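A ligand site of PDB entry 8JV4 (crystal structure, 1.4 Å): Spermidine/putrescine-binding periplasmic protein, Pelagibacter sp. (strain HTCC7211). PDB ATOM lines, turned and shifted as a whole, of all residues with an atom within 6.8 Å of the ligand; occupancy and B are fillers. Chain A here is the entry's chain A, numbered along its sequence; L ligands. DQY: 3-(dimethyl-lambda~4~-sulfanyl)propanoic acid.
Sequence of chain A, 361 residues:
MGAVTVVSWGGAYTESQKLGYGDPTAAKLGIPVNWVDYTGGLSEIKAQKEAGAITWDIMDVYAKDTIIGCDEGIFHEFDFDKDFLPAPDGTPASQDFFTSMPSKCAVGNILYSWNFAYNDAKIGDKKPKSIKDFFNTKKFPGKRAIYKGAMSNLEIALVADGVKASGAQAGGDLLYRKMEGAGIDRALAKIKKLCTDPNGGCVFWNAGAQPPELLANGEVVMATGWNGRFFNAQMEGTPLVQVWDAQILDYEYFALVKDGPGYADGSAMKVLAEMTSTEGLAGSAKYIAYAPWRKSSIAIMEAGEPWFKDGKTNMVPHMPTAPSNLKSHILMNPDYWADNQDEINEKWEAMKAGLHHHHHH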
ATOM      1  N   SER A   8      25.686 -25.112 -36.222  1.00  0.00           N
ATOM      2  CA  SER A   8      26.042 -25.294 -34.817  1.00  0.00           C
ATOM      3  C   SER A   8      27.314 -26.141 -34.723  1.00  0.00           C
ATOM      4  O   SER A   8      28.053 -26.304 -35.699  1.00  0.00           O
ATOM      5  CB  SER A   8      24.840 -25.817 -34.025  1.00  0.00           C
ATOM      6  OG  SER A   8      25.100 -25.715 -32.646  1.00  0.00           O
ATOM      7  N   TRP A   9      27.588 -26.639 -33.508  1.00  0.00           N
ATOM      8  CA  TRP A   9      28.944 -26.977 -33.103  1.00  0.00           C
ATOM      9  C   TRP A   9      29.226 -28.467 -33.101  1.00  0.00           C
ATOM     10  O   TRP A   9      30.332 -28.874 -32.746  1.00  0.00           O
ATOM     11  CB  TRP A   9      29.268 -26.331 -31.742  1.00  0.00           C
ATOM     12  CG  TRP A   9      29.135 -24.840 -31.775  1.00  0.00           C
ATOM     13  CD1 TRP A   9      27.978 -24.106 -31.931  1.00  0.00           C
ATOM     14  CD2 TRP A   9      30.195 -23.883 -31.656  1.00  0.00           C
ATOM     15  NE1 TRP A   9      28.272 -22.770 -31.912  1.00  0.00           N
ATOM     16  CE2 TRP A   9      29.612 -22.596 -31.757  1.00  0.00           C
ATOM     17  CE3 TRP A   9      31.572 -23.977 -31.462  1.00  0.00           C
ATOM     18  CZ2 TRP A   9      30.366 -21.418 -31.663  1.00  0.00           C
ATOM     19  CZ3 TRP A   9      32.322 -22.807 -31.370  1.00  0.00           C
ATOM     20  CH2 TRP A   9      31.705 -21.551 -31.469  1.00  0.00           C
ATOM     21  N   GLY A  10      28.252 -29.284 -33.509  1.00  0.00           N
ATOM     22  CA  GLY A  10      28.458 -30.693 -33.723  1.00  0.00           C
ATOM     23  C   GLY A  10      28.333 -31.528 -32.467  1.00  0.00           C
ATOM     24  O   GLY A  10      28.005 -31.051 -31.371  1.00  0.00           O
ATOM     25  N   ALA A  12      27.673 -33.780 -29.326  1.00  0.00           N
ATOM     26  CA  ALA A  12      26.593 -33.836 -28.353  1.00  0.00           C
ATOM     27  C   ALA A  12      25.797 -32.543 -28.320  1.00  0.00           C
ATOM     28  O   ALA A  12      24.622 -32.560 -27.948  1.00  0.00           O
ATOM     29  CB  ALA A  12      27.178 -34.122 -26.954  1.00  0.00           C
ATOM     30  N   TYR A  13      26.414 -31.425 -28.670  1.00  0.00           N
ATOM     31  CA  TYR A  13      25.690 -30.158 -28.613  1.00  0.00           C
ATOM     32  C   TYR A  13      24.626 -30.089 -29.702  1.00  0.00           C
ATOM     33  O   TYR A  13      23.449 -29.877 -29.413  1.00  0.00           O
ATOM     34  CB  TYR A  13      26.655 -28.964 -28.675  1.00  0.00           C
ATOM     35  CG  TYR A  13      25.920 -27.652 -28.531  1.00  0.00           C
ATOM     36  CD1 TYR A  13      25.184 -27.367 -27.380  1.00  0.00           C
ATOM     37  CD2 TYR A  13      25.914 -26.711 -29.560  1.00  0.00           C
ATOM     38  CE1 TYR A  13      24.492 -26.170 -27.253  1.00  0.00           C
ATOM     39  CE2 TYR A  13      25.230 -25.518 -29.437  1.00  0.00           C
ATOM     40  CZ  TYR A  13      24.509 -25.252 -28.290  1.00  0.00           C
ATOM     41  OH  TYR A  13      23.821 -24.082 -28.132  1.00  0.00           O
ATOM     42  N   THR A  14      25.016 -30.305 -30.963  1.00  0.00           N
ATOM     43  CA  THR A  14      24.005 -30.330 -32.015  1.00  0.00           C
ATOM     44  C   THR A  14      22.936 -31.372 -31.730  1.00  0.00           C
ATOM     45  O   THR A  14      21.750 -31.133 -31.979  1.00  0.00           O
ATOM     46  CB  THR A  14      24.656 -30.531 -33.378  1.00  0.00           C
ATOM     47  OG1 THR A  14      25.396 -29.354 -33.717  1.00  0.00           O
ATOM     48  CG2 THR A  14      23.599 -30.819 -34.470  1.00  0.00           C
ATOM     49  N   GLN A  17      20.321 -30.079 -29.453  1.00  0.00           N
ATOM     50  CA  GLN A  17      19.458 -29.113 -30.117  1.00  0.00           C
ATOM     51  C   GLN A  17      18.464 -29.795 -31.047  1.00  0.00           C
ATOM     52  O   GLN A  17      17.270 -29.487 -31.030  1.00  0.00           O
ATOM     53  CB  GLN A  17      20.316 -28.127 -30.906  1.00  0.00           C
ATOM     54  CG  GLN A  17      21.269 -27.347 -30.039  1.00  0.00           C
ATOM     55  CD  GLN A  17      22.203 -26.489 -30.862  1.00  0.00           C
ATOM     56  OE1 GLN A  17      23.119 -26.999 -31.528  1.00  0.00           O
ATOM     57  NE2 GLN A  17      21.977 -25.179 -30.828  1.00  0.00           N
ATOM     58  N   ASP A  60      24.216 -20.614 -34.533  1.00  0.00           N
ATOM     59  CA  ASP A  60      24.490 -20.696 -33.108  1.00  0.00           C
ATOM     60  C   ASP A  60      25.896 -20.153 -32.906  1.00  0.00           C
ATOM     61  O   ASP A  60      26.856 -20.701 -33.477  1.00  0.00           O
ATOM     62  CB  ASP A  60      24.388 -22.155 -32.671  1.00  0.00           C
ATOM     63  CG  ASP A  60      24.608 -22.348 -31.199  1.00  0.00           C
ATOM     64  OD1 ASP A  60      25.728 -22.025 -30.768  1.00  0.00           O
ATOM     65  OD2 ASP A  60      23.684 -22.800 -30.493  1.00  0.00           O
ATOM     66  N   VAL A  61      25.998 -19.023 -32.192  1.00  0.00           N
ATOM     67  CA  VAL A  61      27.217 -18.222 -32.182  1.00  0.00           C
ATOM     68  C   VAL A  61      27.696 -17.891 -30.771  1.00  0.00           C
ATOM     69  O   VAL A  61      26.901 -17.690 -29.841  1.00  0.00           O
ATOM     70  CB  VAL A  61      27.064 -16.914 -32.974  1.00  0.00           C
ATOM     71  CG1 VAL A  61      26.944 -17.203 -34.451  1.00  0.00           C
ATOM     72  CG2 VAL A  61      25.876 -16.098 -32.471  1.00  0.00           C
ATOM     73  N   TYR A  62      29.020 -17.780 -30.648  1.00  0.00           N
ATOM     74  CA  TYR A  62      29.665 -17.158 -29.499  1.00  0.00           C
ATOM     75  C   TYR A  62      29.043 -15.783 -29.221  1.00  0.00           C
ATOM     76  O   TYR A  62      28.684 -15.028 -30.136  1.00  0.00           O
ATOM     77  CB  TYR A  62      31.130 -16.921 -29.830  1.00  0.00           C
ATOM     78  CG  TYR A  62      32.096 -18.070 -29.676  1.00  0.00           C
ATOM     79  CD1 TYR A  62      32.021 -18.973 -28.626  1.00  0.00           C
ATOM     80  CD2 TYR A  62      33.174 -18.188 -30.546  1.00  0.00           C
ATOM     81  CE1 TYR A  62      32.970 -19.978 -28.470  1.00  0.00           C
ATOM     82  CE2 TYR A  62      34.113 -19.185 -30.394  1.00  0.00           C
ATOM     83  CZ  TYR A  62      34.020 -20.064 -29.349  1.00  0.00           C
ATOM     84  OH  TYR A  62      34.969 -21.046 -29.191  1.00  0.00           O
ATOM     85  N   ASN A 109      20.108 -19.039 -26.231  1.00  0.00           N
ATOM     86  CA  ASN A 109      19.627 -20.414 -26.101  1.00  0.00           C
ATOM     87  C   ASN A 109      20.022 -21.006 -24.761  1.00  0.00           C
ATOM     88  O   ASN A 109      19.145 -21.195 -23.896  1.00  0.00           O
ATOM     89  CB  ASN A 109      19.942 -21.330 -27.298  1.00  0.00           C
ATOM     90  CG  ASN A 109      21.381 -21.238 -27.809  1.00  0.00           C
ATOM     91  OD1 ASN A 109      22.323 -20.972 -27.076  1.00  0.00           O
ATOM     92  ND2 ASN A 109      21.534 -21.491 -29.095  1.00  0.00           N
ATOM     93  N   ILE A 110      21.313 -21.306 -24.540  1.00  0.00           N
ATOM     94  CA  ILE A 110      21.759 -21.934 -23.307  1.00  0.00           C
ATOM     95  C   ILE A 110      22.981 -21.198 -22.743  1.00  0.00           C
ATOM     96  O   ILE A 110      23.604 -20.370 -23.411  1.00  0.00           O
ATOM     97  CB  ILE A 110      22.027 -23.451 -23.458  1.00  0.00           C
ATOM     98  CG1 ILE A 110      23.039 -23.777 -24.568  1.00  0.00           C
ATOM     99  CG2 ILE A 110      20.731 -24.163 -23.762  1.00  0.00           C
ATOM    100  CD1 ILE A 110      24.514 -23.490 -24.247  1.00  0.00           C
ATOM    101  N   TYR A 112      26.734 -22.209 -20.904  1.00  0.00           N
ATOM    102  CA  TYR A 112      27.720 -23.288 -20.858  1.00  0.00           C
ATOM    103  C   TYR A 112      28.932 -22.811 -20.094  1.00  0.00           C
ATOM    104  O   TYR A 112      29.135 -21.606 -19.922  1.00  0.00           O
ATOM    105  CB  TYR A 112      28.130 -23.740 -22.258  1.00  0.00           C
ATOM    106  CG  TYR A 112      28.860 -22.727 -23.113  1.00  0.00           C
ATOM    107  CD1 TYR A 112      28.167 -21.707 -23.760  1.00  0.00           C
ATOM    108  CD2 TYR A 112      30.236 -22.788 -23.303  1.00  0.00           C
ATOM    109  CE1 TYR A 112      28.810 -20.799 -24.567  1.00  0.00           C
ATOM    110  CE2 TYR A 112      30.882 -21.885 -24.101  1.00  0.00           C
ATOM    111  CZ  TYR A 112      30.171 -20.896 -24.737  1.00  0.00           C
ATOM    112  OH  TYR A 112      30.847 -19.995 -25.569  1.00  0.00           O
ATOM    113  N   SER A 113      29.760 -23.768 -19.675  1.00  0.00           N
ATOM    114  CA  SER A 113      31.012 -23.465 -18.985  1.00  0.00           C
ATOM    115  C   SER A 113      32.207 -23.974 -19.778  1.00  0.00           C
ATOM    116  O   SER A 113      32.184 -25.082 -20.325  1.00  0.00           O
ATOM    117  CB  SER A 113      31.061 -24.077 -17.594  1.00  0.00           C
ATOM    118  OG  SER A 113      30.129 -23.468 -16.725  1.00  0.00           O
ATOM    119  N   TRP A 114      33.262 -23.162 -19.774  1.00  0.00           N
ATOM    120  CA  TRP A 114      34.605 -23.634 -20.079  1.00  0.00           C
ATOM    121  C   TRP A 114      35.206 -24.136 -18.771  1.00  0.00           C
ATOM    122  O   TRP A 114      35.249 -23.397 -17.787  1.00  0.00           O
ATOM    123  CB  TRP A 114      35.478 -22.477 -20.586  1.00  0.00           C
ATOM    124  CG  TRP A 114      34.961 -21.692 -21.747  1.00  0.00           C
ATOM    125  CD1 TRP A 114      33.946 -20.781 -21.725  1.00  0.00           C
ATOM    126  CD2 TRP A 114      35.493 -21.677 -23.084  1.00  0.00           C
ATOM    127  NE1 TRP A 114      33.772 -20.216 -22.977  1.00  0.00           N
ATOM    128  CE2 TRP A 114      34.707 -20.748 -23.827  1.00  0.00           C
ATOM    129  CE3 TRP A 114      36.510 -22.370 -23.741  1.00  0.00           C
ATOM    130  CZ2 TRP A 114      34.936 -20.497 -25.170  1.00  0.00           C
ATOM    131  CZ3 TRP A 114      36.737 -22.115 -25.093  1.00  0.00           C
ATOM    132  CH2 TRP A 114      35.937 -21.182 -25.794  1.00  0.00           C
ATOM    133  N   GLY A 208      34.522 -29.134 -30.300  1.00  0.00           N
ATOM    134  CA  GLY A 208      34.116 -29.434 -28.947  1.00  0.00           C
ATOM    135  C   GLY A 208      34.239 -30.894 -28.551  1.00  0.00           C
ATOM    136  O   GLY A 208      34.392 -31.199 -27.371  1.00  0.00           O
ATOM    137  N   TRP A 226      34.344 -27.805 -22.948  1.00  0.00           N
ATOM    138  CA  TRP A 226      33.023 -27.339 -22.570  1.00  0.00           C
ATOM    139  C   TRP A 226      32.338 -28.410 -21.725  1.00  0.00           C
ATOM    140  O   TRP A 226      32.389 -29.595 -22.064  1.00  0.00           O
ATOM    141  CB  TRP A 226      32.217 -26.981 -23.806  1.00  0.00           C
ATOM    142  CG  TRP A 226      32.845 -25.847 -24.575  1.00  0.00           C
ATOM    143  CD1 TRP A 226      33.383 -24.703 -24.060  1.00  0.00           C
ATOM    144  CD2 TRP A 226      33.000 -25.754 -25.998  1.00  0.00           C
ATOM    145  NE1 TRP A 226      33.862 -23.896 -25.078  1.00  0.00           N
ATOM    146  CE2 TRP A 226      33.645 -24.535 -26.275  1.00  0.00           C
ATOM    147  CE3 TRP A 226      32.663 -26.593 -27.073  1.00  0.00           C
ATOM    148  CZ2 TRP A 226      33.944 -24.124 -27.571  1.00  0.00           C
ATOM    149  CZ3 TRP A 226      32.957 -26.183 -28.357  1.00  0.00           C
ATOM    150  CH2 TRP A 226      33.607 -24.972 -28.592  1.00  0.00           C
ATOM    151  N   ASN A 227      31.721 -27.988 -20.625  1.00  0.00           N
ATOM    152  CA  ASN A 227      31.295 -28.955 -19.618  1.00  0.00           C
ATOM    153  C   ASN A 227      30.304 -29.973 -20.170  1.00  0.00           C
ATOM    154  O   ASN A 227      30.282 -31.120 -19.711  1.00  0.00           O
ATOM    155  CB  ASN A 227      30.704 -28.261 -18.385  1.00  0.00           C
ATOM    156  CG  ASN A 227      29.304 -27.720 -18.627  1.00  0.00           C
ATOM    157  OD1 ASN A 227      29.128 -26.651 -19.216  1.00  0.00           O
ATOM    158  ND2 ASN A 227      28.295 -28.475 -18.198  1.00  0.00           N
ATOM    159  N   GLY A 228      29.472 -29.577 -21.129  1.00  0.00           N
ATOM    160  CA  GLY A 228      28.492 -30.504 -21.680  1.00  0.00           C
ATOM    161  C   GLY A 228      29.106 -31.605 -22.512  1.00  0.00           C
ATOM    162  O   GLY A 228      28.539 -32.699 -22.624  1.00  0.00           O
ATOM    163  N   ARG A 229      30.260 -31.337 -23.115  1.00  0.00           N
ATOM    164  CA  ARG A 229      30.967 -32.366 -23.861  1.00  0.00           C
ATOM    165  C   ARG A 229      31.567 -33.385 -22.903  1.00  0.00           C
ATOM    166  O   ARG A 229      31.540 -34.590 -23.172  1.00  0.00           O
ATOM    167  CB  ARG A 229      32.039 -31.736 -24.733  1.00  0.00           C
ATOM    168  CG  ARG A 229      31.510 -30.692 -25.733  1.00  0.00           C
ATOM    169  CD  ARG A 229      30.380 -31.233 -26.638  1.00  0.00           C
ATOM    170  NE  ARG A 229      30.109 -30.206 -27.626  1.00  0.00           N
ATOM    171  CZ  ARG A 229      30.419 -30.256 -28.913  1.00  0.00           C
ATOM    172  NH1 ARG A 229      30.871 -31.360 -29.476  1.00  0.00           N
ATOM    173  NH2 ARG A 229      30.206 -29.179 -29.653  1.00  0.00           N
ATOM    174  N   ASP A 250      29.682 -18.850 -19.577  1.00  0.00           N
ATOM    175  CA  ASP A 250      29.507 -18.188 -20.857  1.00  0.00           C
ATOM    176  C   ASP A 250      28.076 -18.397 -21.313  1.00  0.00           C
ATOM    177  O   ASP A 250      27.364 -19.283 -20.828  1.00  0.00           O
ATOM    178  CB  ASP A 250      30.549 -18.749 -21.848  1.00  0.00           C
ATOM    179  CG  ASP A 250      30.943 -17.775 -22.949  1.00  0.00           C
ATOM    180  OD1 ASP A 250      30.185 -16.821 -23.248  1.00  0.00           O
ATOM    181  OD2 ASP A 250      32.046 -17.983 -23.510  1.00  0.00           O
ATOM    182  N   GLU A 252      25.402 -18.560 -24.701  1.00  0.00           N
ATOM    183  CA  GLU A 252      25.341 -18.855 -26.126  1.00  0.00           C
ATOM    184  C   GLU A 252      24.044 -18.307 -26.714  1.00  0.00           C
ATOM    185  O   GLU A 252      23.040 -18.095 -26.001  1.00  0.00           O
ATOM    186  CB  GLU A 252      25.472 -20.351 -26.380  1.00  0.00           C
ATOM    187  CG  GLU A 252      25.793 -20.752 -27.809  1.00  0.00           C
ATOM    188  CD  GLU A 252      27.187 -20.395 -28.277  1.00  0.00           C
ATOM    189  OE1 GLU A 252      27.950 -19.812 -27.503  1.00  0.00           O
ATOM    190  OE2 GLU A 252      27.497 -20.705 -29.463  1.00  0.00           O
ATOM    191  N   ILE A 288      21.722 -32.600 -22.461  1.00  0.00           N
ATOM    192  CA  ILE A 288      23.073 -32.116 -22.183  1.00  0.00           C
ATOM    193  C   ILE A 288      22.990 -31.136 -21.016  1.00  0.00           C
ATOM    194  O   ILE A 288      21.974 -30.463 -20.796  1.00  0.00           O
ATOM    195  CB  ILE A 288      23.686 -31.490 -23.459  1.00  0.00           C
ATOM    196  CG1 ILE A 288      25.197 -31.350 -23.337  1.00  0.00           C
ATOM    197  CG2 ILE A 288      23.022 -30.147 -23.766  1.00  0.00           C
ATOM    198  CD1 ILE A 288      25.859 -31.098 -24.661  1.00  0.00           C
ATOM    199  N   TYR A 290      23.570 -28.113 -20.138  1.00  0.00           N
ATOM    200  CA  TYR A 290      23.613 -26.685 -20.386  1.00  0.00           C
ATOM    201  C   TYR A 290      22.298 -26.082 -19.932  1.00  0.00           C
ATOM    202  O   TYR A 290      21.225 -26.681 -20.107  1.00  0.00           O
ATOM    203  CB  TYR A 290      23.879 -26.360 -21.876  1.00  0.00           C
ATOM    204  CG  TYR A 290      25.247 -26.772 -22.367  1.00  0.00           C
ATOM    205  CD1 TYR A 290      26.355 -26.685 -21.545  1.00  0.00           C
ATOM    206  CD2 TYR A 290      25.428 -27.274 -23.648  1.00  0.00           C
ATOM    207  CE1 TYR A 290      27.607 -27.056 -21.969  1.00  0.00           C
ATOM    208  CE2 TYR A 290      26.686 -27.651 -24.100  1.00  0.00           C
ATOM    209  CZ  TYR A 290      27.768 -27.547 -23.249  1.00  0.00           C
ATOM    210  OH  TYR A 290      29.026 -27.933 -23.648  1.00  0.00           O
HETATM  211  S   DQY L   1      29.854 -24.077 -28.202  1.00  0.00           S
HETATM  212  C1  DQY L   1      29.165 -26.938 -26.899  1.00  0.00           C
HETATM  213  O1  DQY L   1      29.316 -26.860 -28.128  1.00  0.00           O
HETATM  214  C2  DQY L   1      28.866 -25.663 -26.130  1.00  0.00           C
HETATM  215  O2  DQY L   1      29.215 -28.021 -26.246  1.00  0.00           O
HETATM  216  C3  DQY L   1      29.794 -24.499 -26.460  1.00  0.00           C
HETATM  217  CM1 DQY L   1      28.157 -23.813 -28.576  1.00  0.00           C
HETATM  218  CM2 DQY L   1      30.532 -22.428 -28.140  1.00  0.00           C
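O2 of the ligand sits at hydrogen-bond distance from OH of Tyr 290, at 2.6 Å.
The guanidinium group of Arg 229 lies within salt-bridge range of an oxygen (O2) of the ligand (2.7 Å).
The side-chain hydroxyl (OH) of Tyr 290 lies within hydrogen-bond range of the backbone NH (N) of Gly 228 (3.0 Å).
The backbone carbonyl oxygen (O) of Trp 9 is in hydrogen-bond range of the guanidinium group (NH2) of Arg 229.
The side-chain hydroxyl of Tyr 112 lies close to the side-chain carboxylate of Glu 252 (3.5 Å).
The backbone NH (N) of Asn 109 lies within hydrogen-bond range of the backbone carbonyl oxygen (O) of Glu 252, at 3.1 Å.
N of Trp 9 is in hydrogen-bond range of OG1 of Thr 14.
OH of Tyr 13 sits at hydrogen-bond distance from NE2 of Gln 17 (3.4 Å).
The side-chain carboxylate (OD2) of Asp 60 sits at hydrogen-bond distance from the side-chain amide nitrogen (NE2) of Gln 17.
OD2 of Asp 60 sits at hydrogen-bond distance from ND2 of Asn 109, 2.9 Å away.
Trp 9 touches the ligand.
Tyr 13 touches the ligand.
OD1 of Asp 60 touches CM1 of the ligand, at 3.7 Å.
Tyr 62 touches the ligand (CE1 to CM2, 3.5 Å).
Tyr 112 touches the ligand (OH to CM2, 3.6 Å).
CD2 of Trp 226 touches C3 of the ligand, 3.5 Å away.
OE2 of Glu 252 touches CM1 of the ligand, at 3.3 Å.
Within 4 Å of the ligand: Trp 9, Tyr 13, Asp 60, Tyr 62, Tyr 112, Trp 226, Arg 229, Glu 252 and Tyr 290.
The nearest printed residue that does not touch the ligand is Ile 288 (4.8 Å).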
